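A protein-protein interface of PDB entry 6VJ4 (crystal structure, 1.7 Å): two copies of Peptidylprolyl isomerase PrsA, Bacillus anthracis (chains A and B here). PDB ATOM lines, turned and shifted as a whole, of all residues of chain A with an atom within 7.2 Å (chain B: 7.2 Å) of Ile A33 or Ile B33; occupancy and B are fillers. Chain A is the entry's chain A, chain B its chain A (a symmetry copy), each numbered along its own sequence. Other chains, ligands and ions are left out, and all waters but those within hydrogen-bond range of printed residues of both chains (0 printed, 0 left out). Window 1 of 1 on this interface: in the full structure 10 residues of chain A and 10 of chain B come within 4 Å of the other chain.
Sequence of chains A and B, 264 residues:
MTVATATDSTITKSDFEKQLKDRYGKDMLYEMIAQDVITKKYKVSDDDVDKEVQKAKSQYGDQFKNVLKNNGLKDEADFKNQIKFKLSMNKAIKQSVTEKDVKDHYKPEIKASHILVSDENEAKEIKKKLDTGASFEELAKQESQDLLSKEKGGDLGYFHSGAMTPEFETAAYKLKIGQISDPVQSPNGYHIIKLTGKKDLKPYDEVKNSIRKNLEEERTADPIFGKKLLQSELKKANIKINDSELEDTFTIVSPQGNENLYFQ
The side-chain sulfur of Met A32 sits close to the side-chain carboxylate of Asp B36. The side-chain sulfur (SD) of Met B32 sits close to the side-chain carboxylate (OD2) of Asp A36, 3.6 Å away. The side-chain carboxylate (OD2) of Asp A36 lies close to the side-chain carboxylate (OD2) of Asp B36 (2.7 Å).
OG1 of Thr A39 sits at hydrogen-bond distance from O of Asp A36, at 3.2 Å. O of Leu B234 sits at hydrogen-bond distance from N of Ile B239, at 3.2 Å. O of Asp B36 is in hydrogen-bond range of OG1 of Thr B39 (3.2 Å). The side-chain carboxylate (OD1) of Asp B36 lies close to the backbone carbonyl oxygen (O) of Met B32, 2.7 Å away. The backbone carbonyl oxygen (O) of Met A32 sits close to the side-chain carboxylate (OD1) of Asp A36. The backbone carbonyl oxygen of Leu A234 lies within hydrogen-bond range of the backbone NH of Ile A239, at 3.2 Å.
Among the printed residues, pairs that only touch across the chains: Ile A239 with Ile B33, Ile A33 with Ile B239, Leu A29 with Ala B237, Ala A237 with Leu B29, Ile A33 with Ile B33 and Ile A239 with Ile B239.
Of the printed residues of chain B, Leu A29 touches Ala B237 (3.3 Å). Of the printed residues of chain A, Asp B36 touches Met A32 (3.4 Å) and Asp A36 (2.7 Å). The nearest residue of chain B that does not touch Ile A33 is Val B37 (4.1 Å). The nearest residue of chain A that does not touch Ile B33 is Val A37 (4.1 Å).
Of the 17 printed residues of chain A, 6 touch a printed residue of chain B. Printed residues of chain A that touch a printed residue of chain B: Leu A29, Met A32, Ile A33, Asp A36, Ala A237 and Ile A239. Hydrophobic or aromatic side chains of chain A that line the printed part of chain B: Leu A29, Met A32, Ile A33, Ala A237 and Ile A239. Hydrophobic or aromatic side chains of chain B that line the printed part of chain A: Leu B29, Met B32, Ile B33, Ala B237 and Ile B239.
Leu A29 touches Ala B237, and with the chains exchanged Ala A237 touches Leu B29. Met A32 touches Asp B36, and with the chains exchanged Asp A36 touches Met B32. Ile A33 touches Ile B239, and with the chains exchanged Ile A239 touches Ile B33. Asp B36 touches its own counterpart, Asp A36. Positions printed for both chains: 28, 29, 30, 31, 32, 33, 34, 35, 36, 37, 38, 39, 230, 234, 237, 239 and 241.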
ATOM      1  N   MET A  28      14.407   9.447  11.896  1.00  0.00           N
ATOM      2  CA  MET A  28      15.544   9.820  11.068  1.00  0.00           C
ATOM      3  C   MET A  28      16.277  11.004  11.699  1.00  0.00           C
ATOM      4  O   MET A  28      17.434  11.261  11.370  1.00  0.00           O
ATOM      5  CB  MET A  28      15.083  10.164   9.646  1.00  0.00           C
ATOM      6  CG  MET A  28      14.901   8.961   8.738  1.00  0.00           C
ATOM      7  SD  MET A  28      16.498   7.809   8.702  1.00  0.00           S
ATOM      8  CE  MET A  28      17.799   8.411   7.366  1.00  0.00           C
ATOM      9  N   LEU A  29      15.588  11.724  12.594  1.00  0.00           N
ATOM     10  CA  LEU A  29      16.183  12.854  13.288  1.00  0.00           C
ATOM     11  C   LEU A  29      16.953  12.339  14.510  1.00  0.00           C
ATOM     12  O   LEU A  29      18.092  12.801  14.730  1.00  0.00           O
ATOM     13  CB  LEU A  29      15.078  13.827  13.705  1.00  0.00           C
ATOM     14  CG  LEU A  29      15.554  15.097  14.407  1.00  0.00           C
ATOM     15  CD1 LEU A  29      16.476  15.907  13.506  1.00  0.00           C
ATOM     16  CD2 LEU A  29      14.372  15.942  14.853  1.00  0.00           C
ATOM     17  N   TYR A  30      16.335  11.432  15.276  1.00  0.00           N
ATOM     18  CA  TYR A  30      16.980  10.817  16.468  1.00  0.00           C
ATOM     19  C   TYR A  30      18.352  10.269  16.063  1.00  0.00           C
ATOM     20  O   TYR A  30      19.331  10.497  16.799  1.00  0.00           O
ATOM     21  CB  TYR A  30      16.070   9.735  17.058  1.00  0.00           C
ATOM     22  CG  TYR A  30      16.720   8.807  18.058  1.00  0.00           C
ATOM     23  CD1 TYR A  30      16.968   9.211  19.360  1.00  0.00           C
ATOM     24  CD2 TYR A  30      17.051   7.506  17.712  1.00  0.00           C
ATOM     25  CE1 TYR A  30      17.553   8.359  20.284  1.00  0.00           C
ATOM     26  CE2 TYR A  30      17.631   6.638  18.624  1.00  0.00           C
ATOM     27  CZ  TYR A  30      17.884   7.068  19.915  1.00  0.00           C
ATOM     28  OH  TYR A  30      18.455   6.218  20.817  1.00  0.00           O
ATOM     29  N   GLU A  31      18.407   9.596  14.908  1.00  0.00           N
ATOM     30  CA  GLU A  31      19.657   8.996  14.367  1.00  0.00           C
ATOM     31  C   GLU A  31      20.716  10.086  14.212  1.00  0.00           C
ATOM     32  O   GLU A  31      21.804   9.987  14.774  1.00  0.00           O
ATOM     33  CB  GLU A  31      19.365   8.300  13.034  1.00  0.00           C
ATOM     34  CG  GLU A  31      20.556   7.564  12.444  1.00  0.00           C
ATOM     35  CD  GLU A  31      20.265   6.827  11.146  1.00  0.00           C
ATOM     36  OE1 GLU A  31      19.173   7.034  10.578  1.00  0.00           O
ATOM     37  OE2 GLU A  31      21.126   6.037  10.710  1.00  0.00           O
ATOM     38  N   MET A  32      20.372  11.136  13.459  1.00  0.00           N
ATOM     39  CA  MET A  32      21.277  12.244  13.204  1.00  0.00           C
ATOM     40  C   MET A  32      21.872  12.755  14.515  1.00  0.00           C
ATOM     41  O   MET A  32      23.089  12.841  14.651  1.00  0.00           O
ATOM     42  CB  MET A  32      20.530  13.370  12.484  1.00  0.00           C
ATOM     43  CG  MET A  32      21.374  14.586  12.173  1.00  0.00           C
ATOM     44  SD  MET A  32      20.281  15.965  11.302  1.00  0.00           S
ATOM     45  CE  MET A  32      20.537  15.876   9.352  1.00  0.00           C
ATOM     46  N   ILE A  33      20.996  13.089  15.470  1.00  0.00           N
ATOM     47  CA  ILE A  33      21.405  13.628  16.758  1.00  0.00           C
ATOM     48  C   ILE A  33      22.247  12.597  17.522  1.00  0.00           C
ATOM     49  O   ILE A  33      23.390  12.937  17.906  1.00  0.00           O
ATOM     50  CB  ILE A  33      20.171  14.080  17.565  1.00  0.00           C
ATOM     51  CG1 ILE A  33      19.484  15.269  16.890  1.00  0.00           C
ATOM     52  CG2 ILE A  33      20.549  14.384  19.009  1.00  0.00           C
ATOM     53  CD1 ILE A  33      18.245  15.756  17.596  1.00  0.00           C
ATOM     54  N   ALA A  34      21.698  11.396  17.739  1.00  0.00           N
ATOM     55  CA  ALA A  34      22.406  10.328  18.486  1.00  0.00           C
ATOM     56  C   ALA A  34      23.797  10.103  17.883  1.00  0.00           C
ATOM     57  O   ALA A  34      24.765   9.958  18.662  1.00  0.00           O
ATOM     58  CB  ALA A  34      21.588   9.060  18.470  1.00  0.00           C
ATOM     59  N   GLN A  35      23.888  10.101  16.549  1.00  0.00           N
ATOM     60  CA  GLN A  35      25.180   9.877  15.845  1.00  0.00           C
ATOM     61  C   GLN A  35      26.078  11.110  16.015  1.00  0.00           C
ATOM     62  O   GLN A  35      27.301  10.921  16.166  1.00  0.00           O
ATOM     63  CB  GLN A  35      24.947   9.546  14.368  1.00  0.00           C
ATOM     64  CG  GLN A  35      24.253   8.206  14.142  1.00  0.00           C
ATOM     65  CD  GLN A  35      24.221   7.781  12.693  1.00  0.00           C
ATOM     66  OE1 GLN A  35      24.714   8.474  11.804  1.00  0.00           O
ATOM     67  NE2 GLN A  35      23.641   6.618  12.446  1.00  0.00           N
ATOM     68  N   ASP A  36      25.495  12.314  16.007  1.00  0.00           N
ATOM     69  CA  ASP A  36      26.297  13.562  16.152  1.00  0.00           C
ATOM     70  C   ASP A  36      26.971  13.608  17.530  1.00  0.00           C
ATOM     71  O   ASP A  36      28.139  14.035  17.595  1.00  0.00           O
ATOM     72  CB  ASP A  36      25.451  14.818  15.918  1.00  0.00           C
ATOM     73  CG  ASP A  36      25.258  15.173  14.453  1.00  0.00           C
ATOM     74  OD1 ASP A  36      25.100  14.238  13.636  1.00  0.00           O
ATOM     75  OD2 ASP A  36      25.291  16.380  14.134  1.00  0.00           O
ATOM     76  N   VAL A  37      26.255  13.213  18.586  1.00  0.00           N
ATOM     77  CA  VAL A  37      26.823  13.231  19.969  1.00  0.00           C
ATOM     78  C   VAL A  37      28.026  12.280  20.028  1.00  0.00           C
ATOM     79  O   VAL A  37      29.095  12.717  20.489  1.00  0.00           O
ATOM     80  CB  VAL A  37      25.758  12.862  21.019  1.00  0.00           C
ATOM     81  CG1 VAL A  37      26.356  12.716  22.412  1.00  0.00           C
ATOM     82  CG2 VAL A  37      24.615  13.866  21.031  1.00  0.00           C
ATOM     83  N   ILE A  38      27.859  11.041  19.553  1.00  0.00           N
ATOM     84  CA  ILE A  38      28.956  10.026  19.595  1.00  0.00           C
ATOM     85  C   ILE A  38      30.111  10.447  18.680  1.00  0.00           C
ATOM     86  O   ILE A  38      31.266  10.438  19.155  1.00  0.00           O
ATOM     87  CB  ILE A  38      28.411   8.636  19.215  1.00  0.00           C
ATOM     88  CG1 ILE A  38      27.308   8.198  20.178  1.00  0.00           C
ATOM     89  CG2 ILE A  38      29.531   7.609  19.124  1.00  0.00           C
ATOM     90  CD1 ILE A  38      27.712   8.234  21.637  1.00  0.00           C
ATOM     91  N   THR A  39      29.808  10.816  17.432  1.00  0.00           N
ATOM     92  CA  THR A  39      30.865  11.168  16.441  1.00  0.00           C
ATOM     93  C   THR A  39      31.622  12.430  16.868  1.00  0.00           C
ATOM     94  O   THR A  39      32.787  12.566  16.455  1.00  0.00           O
ATOM     95  CB  THR A  39      30.275  11.318  15.033  1.00  0.00           C
ATOM     96  OG1 THR A  39      29.229  12.288  15.088  1.00  0.00           O
ATOM     97  CG2 THR A  39      29.743  10.013  14.485  1.00  0.00           C
ATOM     98  N   LEU A 230      24.721   4.718  24.705  1.00  0.00           N
ATOM     99  CA  LEU A 230      24.213   5.878  23.925  1.00  0.00           C
ATOM    100  C   LEU A 230      23.262   6.701  24.807  1.00  0.00           C
ATOM    101  O   LEU A 230      23.449   7.930  24.880  1.00  0.00           O
ATOM    102  CB  LEU A 230      23.523   5.365  22.657  1.00  0.00           C
ATOM    103  CG  LEU A 230      22.901   6.431  21.752  1.00  0.00           C
ATOM    104  CD1 LEU A 230      23.897   7.531  21.418  1.00  0.00           C
ATOM    105  CD2 LEU A 230      22.357   5.798  20.481  1.00  0.00           C
ATOM    106  N   LEU A 234      23.840  10.654  25.908  1.00  0.00           N
ATOM    107  CA  LEU A 234      22.864  11.751  25.671  1.00  0.00           C
ATOM    108  C   LEU A 234      22.516  12.398  27.019  1.00  0.00           C
ATOM    109  O   LEU A 234      22.437  13.639  27.071  1.00  0.00           O
ATOM    110  CB  LEU A 234      21.612  11.191  24.988  1.00  0.00           C
ATOM    111  CG  LEU A 234      21.833  10.519  23.631  1.00  0.00           C
ATOM    112  CD1 LEU A 234      20.537   9.918  23.107  1.00  0.00           C
ATOM    113  CD2 LEU A 234      22.411  11.496  22.621  1.00  0.00           C
ATOM    114  N   ALA A 237      24.974  14.714  28.262  1.00  0.00           N
ATOM    115  CA  ALA A 237      24.894  15.945  27.436  1.00  0.00           C
ATOM    116  C   ALA A 237      23.607  16.728  27.746  1.00  0.00           C
ATOM    117  O   ALA A 237      23.388  17.761  27.088  1.00  0.00           O
ATOM    118  CB  ALA A 237      24.975  15.582  25.973  1.00  0.00           C
ATOM    119  N   ILE A 239      20.165  15.800  27.406  1.00  0.00           N
ATOM    120  CA  ILE A 239      19.249  15.676  26.231  1.00  0.00           C
ATOM    121  C   ILE A 239      18.296  14.502  26.478  1.00  0.00           C
ATOM    122  O   ILE A 239      18.797  13.374  26.648  1.00  0.00           O
ATOM    123  CB  ILE A 239      20.049  15.468  24.928  1.00  0.00           C
ATOM    124  CG1 ILE A 239      21.123  16.541  24.730  1.00  0.00           C
ATOM    125  CG2 ILE A 239      19.113  15.377  23.731  1.00  0.00           C
ATOM    126  CD1 ILE A 239      22.037  16.287  23.556  1.00  0.00           C
ATOM    127  N   ILE A 241      15.358  12.117  24.888  1.00  0.00           N
ATOM    128  CA  ILE A 241      14.724  11.677  23.606  1.00  0.00           C
ATOM    129  C   ILE A 241      13.932  10.390  23.873  1.00  0.00           C
ATOM    130  O   ILE A 241      14.120   9.793  24.952  1.00  0.00           O
ATOM    131  CB  ILE A 241      15.777  11.474  22.497  1.00  0.00           C
ATOM    132  CG1 ILE A 241      16.812  12.604  22.464  1.00  0.00           C
ATOM    133  CG2 ILE A 241      15.094  11.288  21.148  1.00  0.00           C
ATOM    134  CD1 ILE A 241      17.924  12.396  21.462  1.00  0.00           C
ATOM    135  N   MET B  28      28.572  23.805  22.891  1.00  0.00           N
ATOM    136  CA  MET B  28      28.993  23.582  21.516  1.00  0.00           C
ATOM    137  C   MET B  28      28.230  22.396  20.928  1.00  0.00           C
ATOM    138  O   MET B  28      28.168  22.244  19.708  1.00  0.00           O
ATOM    139  CB  MET B  28      30.506  23.340  21.450  1.00  0.00           C
ATOM    140  CG  MET B  28      31.344  24.606  21.431  1.00  0.00           C
ATOM    141  SD  MET B  28      30.768  25.856  20.023  1.00  0.00           S
ATOM    142  CE  MET B  28      31.627  25.463  18.306  1.00  0.00           C
ATOM    143  N   LEU B  29      27.666  21.555  21.805  1.00  0.00           N
ATOM    144  CA  LEU B  29      26.887  20.407  21.372  1.00  0.00           C
ATOM    145  C   LEU B  29      25.447  20.858  21.097  1.00  0.00           C
ATOM    146  O   LEU B  29      24.887  20.451  20.057  1.00  0.00           O
ATOM    147  CB  LEU B  29      26.928  19.331  22.459  1.00  0.00           C
ATOM    148  CG  LEU B  29      26.190  18.036  22.128  1.00  0.00           C
ATOM    149  CD1 LEU B  29      26.780  17.372  20.892  1.00  0.00           C
ATOM    150  CD2 LEU B  29      26.220  17.080  23.309  1.00  0.00           C
ATOM    151  N   TYR B  30      24.876  21.650  22.012  1.00  0.00           N
ATOM    152  CA  TYR B  30      23.500  22.194  21.854  1.00  0.00           C
ATOM    153  C   TYR B  30      23.386  22.864  20.480  1.00  0.00           C
ATOM    154  O   TYR B  30      22.380  22.634  19.782  1.00  0.00           O
ATOM    155  CB  TYR B  30      23.182  23.158  23.001  1.00  0.00           C
ATOM    156  CG  TYR B  30      21.964  24.031  22.803  1.00  0.00           C
ATOM    157  CD1 TYR B  30      20.683  23.528  22.962  1.00  0.00           C
ATOM    158  CD2 TYR B  30      22.095  25.377  22.496  1.00  0.00           C
ATOM    159  CE1 TYR B  30      19.564  24.329  22.794  1.00  0.00           C
ATOM    160  CE2 TYR B  30      20.988  26.194  22.330  1.00  0.00           C
ATOM    161  CZ  TYR B  30      19.717  25.667  22.478  1.00  0.00           C
ATOM    162  OH  TYR B  30      18.624  26.465  22.315  1.00  0.00           O
ATOM    163  N   GLU B  31      24.410  23.640  20.109  1.00  0.00           N
ATOM    164  CA  GLU B  31      24.460  24.366  18.811  1.00  0.00           C
ATOM    165  C   GLU B  31      24.321  23.365  17.665  1.00  0.00           C
ATOM    166  O   GLU B  31      23.422  23.482  16.837  1.00  0.00           O
ATOM    167  CB  GLU B  31      25.767  25.160  18.710  1.00  0.00           C
ATOM    168  CG  GLU B  31      25.875  26.021  17.462  1.00  0.00           C
ATOM    169  CD  GLU B  31      27.146  26.853  17.376  1.00  0.00           C
ATOM    170  OE1 GLU B  31      28.059  26.628  18.196  1.00  0.00           O
ATOM    171  OE2 GLU B  31      27.215  27.732  16.494  1.00  0.00           O
ATOM    172  N   MET B  32      25.211  22.368  17.647  1.00  0.00           N
ATOM    173  CA  MET B  32      25.218  21.347  16.612  1.00  0.00           C
ATOM    174  C   MET B  32      23.819  20.759  16.437  1.00  0.00           C
ATOM    175  O   MET B  32      23.289  20.739  15.331  1.00  0.00           O
ATOM    176  CB  MET B  32      26.218  20.245  16.974  1.00  0.00           C
ATOM    177  CG  MET B  32      26.305  19.119  15.969  1.00  0.00           C
ATOM    178  SD  MET B  32      27.578  17.758  16.585  1.00  0.00           S
ATOM    179  CE  MET B  32      29.320  18.039  15.710  1.00  0.00           C
ATOM    180  N   ILE B  33      23.237  20.284  17.545  1.00  0.00           N
ATOM    181  CA  ILE B  33      21.924  19.658  17.535  1.00  0.00           C
ATOM    182  C   ILE B  33      20.857  20.667  17.089  1.00  0.00           C
ATOM    183  O   ILE B  33      20.135  20.368  16.110  1.00  0.00           O
ATOM    184  CB  ILE B  33      21.608  19.057  18.920  1.00  0.00           C
ATOM    185  CG1 ILE B  33      22.549  17.892  19.236  1.00  0.00           C
ATOM    186  CG2 ILE B  33      20.143  18.648  19.013  1.00  0.00           C
ATOM    187  CD1 ILE B  33      22.332  17.265  20.589  1.00  0.00           C
ATOM    188  N   ALA B  34      20.761  21.806  17.785  1.00  0.00           N
ATOM    189  CA  ALA B  34      19.753  22.845  17.463  1.00  0.00           C
ATOM    190  C   ALA B  34      19.838  23.212  15.977  1.00  0.00           C
ATOM    191  O   ALA B  34      18.772  23.348  15.336  1.00  0.00           O
ATOM    192  CB  ALA B  34      19.960  24.055  18.340  1.00  0.00           C
ATOM    193  N   GLN B  35      21.062  23.341  15.452  1.00  0.00           N
ATOM    194  CA  GLN B  35      21.275  23.710  14.026  1.00  0.00           C
ATOM    195  C   GLN B  35      20.894  22.528  13.126  1.00  0.00           C
ATOM    196  O   GLN B  35      20.329  22.779  12.044  1.00  0.00           O
ATOM    197  CB  GLN B  35      22.721  24.158  13.789  1.00  0.00           C
ATOM    198  CG  GLN B  35      23.081  25.466  14.489  1.00  0.00           C
ATOM    199  CD  GLN B  35      24.426  26.018  14.081  1.00  0.00           C
ATOM    200  OE1 GLN B  35      25.140  25.441  13.261  1.00  0.00           O
ATOM    201  NE2 GLN B  35      24.778  27.158  14.649  1.00  0.00           N
ATOM    202  N   ASP B  36      21.174  21.294  13.563  1.00  0.00           N
ATOM    203  CA  ASP B  36      20.848  20.091  12.744  1.00  0.00           C
ATOM    204  C   ASP B  36      19.330  19.964  12.560  1.00  0.00           C
ATOM    205  O   ASP B  36      18.905  19.609  11.445  1.00  0.00           O
ATOM    206  CB  ASP B  36      21.432  18.810  13.348  1.00  0.00           C
ATOM    207  CG  ASP B  36      22.897  18.578  13.016  1.00  0.00           C
ATOM    208  OD1 ASP B  36      23.658  19.571  12.979  1.00  0.00           O
ATOM    209  OD2 ASP B  36      23.263  17.409  12.770  1.00  0.00           O
ATOM    210  N   VAL B  37      18.553  20.215  13.616  1.00  0.00           N
ATOM    211  CA  VAL B  37      17.064  20.109  13.536  1.00  0.00           C
ATOM    212  C   VAL B  37      16.544  21.126  12.511  1.00  0.00           C
ATOM    213  O   VAL B  37      15.780  20.718  11.618  1.00  0.00           O
ATOM    214  CB  VAL B  37      16.410  20.312  14.916  1.00  0.00           C
ATOM    215  CG1 VAL B  37      14.891  20.369  14.826  1.00  0.00           C
ATOM    216  CG2 VAL B  37      16.846  19.241  15.904  1.00  0.00           C
ATOM    217  N   ILE B  38      16.967  22.389  12.624  1.00  0.00           N
ATOM    218  CA  ILE B  38      16.495  23.464  11.698  1.00  0.00           C
ATOM    219  C   ILE B  38      16.994  23.202  10.273  1.00  0.00           C
ATOM    220  O   ILE B  38      16.159  23.242   9.345  1.00  0.00           O
ATOM    221  CB  ILE B  38      16.945  24.846  12.211  1.00  0.00           C
ATOM    222  CG1 ILE B  38      16.382  25.123  13.605  1.00  0.00           C
ATOM    223  CG2 ILE B  38      16.589  25.946  11.222  1.00  0.00           C
ATOM    224  CD1 ILE B  38      14.878  24.981  13.702  1.00  0.00           C
ATOM    225  N   THR B  39      18.292  22.930  10.113  1.00  0.00           N
ATOM    226  CA  THR B  39      18.891  22.737   8.762  1.00  0.00           C
ATOM    227  C   THR B  39      18.318  21.493   8.077  1.00  0.00           C
ATOM    228  O   THR B  39      18.323  21.470   6.834  1.00  0.00           O
ATOM    229  CB  THR B  39      20.423  22.678   8.840  1.00  0.00           C
ATOM    230  OG1 THR B  39      20.784  21.642   9.753  1.00  0.00           O
ATOM    231  CG2 THR B  39      21.033  23.990   9.277  1.00  0.00           C
ATOM    232  N   LEU B 230      12.771  28.005  17.841  1.00  0.00           N
ATOM    233  CA  LEU B 230      13.749  26.891  17.957  1.00  0.00           C
ATOM    234  C   LEU B 230      13.292  25.933  19.067  1.00  0.00           C
ATOM    235  O   LEU B 230      13.240  24.716  18.803  1.00  0.00           O
ATOM    236  CB  LEU B 230      15.140  27.471  18.235  1.00  0.00           C
ATOM    237  CG  LEU B 230      16.267  26.454  18.425  1.00  0.00           C
ATOM    238  CD1 LEU B 230      16.318  25.455  17.279  1.00  0.00           C
ATOM    239  CD2 LEU B 230      17.604  27.163  18.575  1.00  0.00           C
ATOM    240  N   LEU B 234      12.317  21.942  18.528  1.00  0.00           N
ATOM    241  CA  LEU B 234      12.937  20.809  19.268  1.00  0.00           C
ATOM    242  C   LEU B 234      11.828  20.022  19.980  1.00  0.00           C
ATOM    243  O   LEU B 234      11.885  18.780  19.959  1.00  0.00           O
ATOM    244  CB  LEU B 234      13.963  21.348  20.270  1.00  0.00           C
ATOM    245  CG  LEU B 234      15.121  22.153  19.677  1.00  0.00           C
ATOM    246  CD1 LEU B 234      16.009  22.715  20.778  1.00  0.00           C
ATOM    247  CD2 LEU B 234      15.940  21.310  18.713  1.00  0.00           C
ATOM    248  N   ALA B 237       9.984  17.766  17.870  1.00  0.00           N
ATOM    249  CA  ALA B 237      10.865  16.612  17.561  1.00  0.00           C
ATOM    250  C   ALA B 237      11.056  15.724  18.802  1.00  0.00           C
ATOM    251  O   ALA B 237      11.814  14.742  18.698  1.00  0.00           O
ATOM    252  CB  ALA B 237      12.191  17.110  17.037  1.00  0.00           C
ATOM    253  N   ILE B 239      12.471  16.456  22.010  1.00  0.00           N
ATOM    254  CA  ILE B 239      13.874  16.627  22.495  1.00  0.00           C
ATOM    255  C   ILE B 239      13.886  17.711  23.579  1.00  0.00           C
ATOM    256  O   ILE B 239      13.487  18.848  23.265  1.00  0.00           O
ATOM    257  CB  ILE B 239      14.817  17.003  21.333  1.00  0.00           C
ATOM    258  CG1 ILE B 239      14.712  16.023  20.161  1.00  0.00           C
ATOM    259  CG2 ILE B 239      16.250  17.142  21.827  1.00  0.00           C
ATOM    260  CD1 ILE B 239      15.492  16.440  18.938  1.00  0.00           C
ATOM    261  N   ILE B 241      16.213  20.036  26.032  1.00  0.00           N
ATOM    262  CA  ILE B 241      17.602  20.549  26.246  1.00  0.00           C
ATOM    263  C   ILE B 241      17.535  21.753  27.194  1.00  0.00           C
ATOM    264  O   ILE B 241      16.419  22.261  27.427  1.00  0.00           O
ATOM    265  CB  ILE B 241      18.279  20.918  24.910  1.00  0.00           C
ATOM    266  CG1 ILE B 241      18.035  19.865  23.824  1.00  0.00           C
ATOM    267  CG2 ILE B 241      19.764  21.181  25.124  1.00  0.00           C
ATOM    268  CD1 ILE B 241      18.591  20.234  22.467  1.00  0.00           C
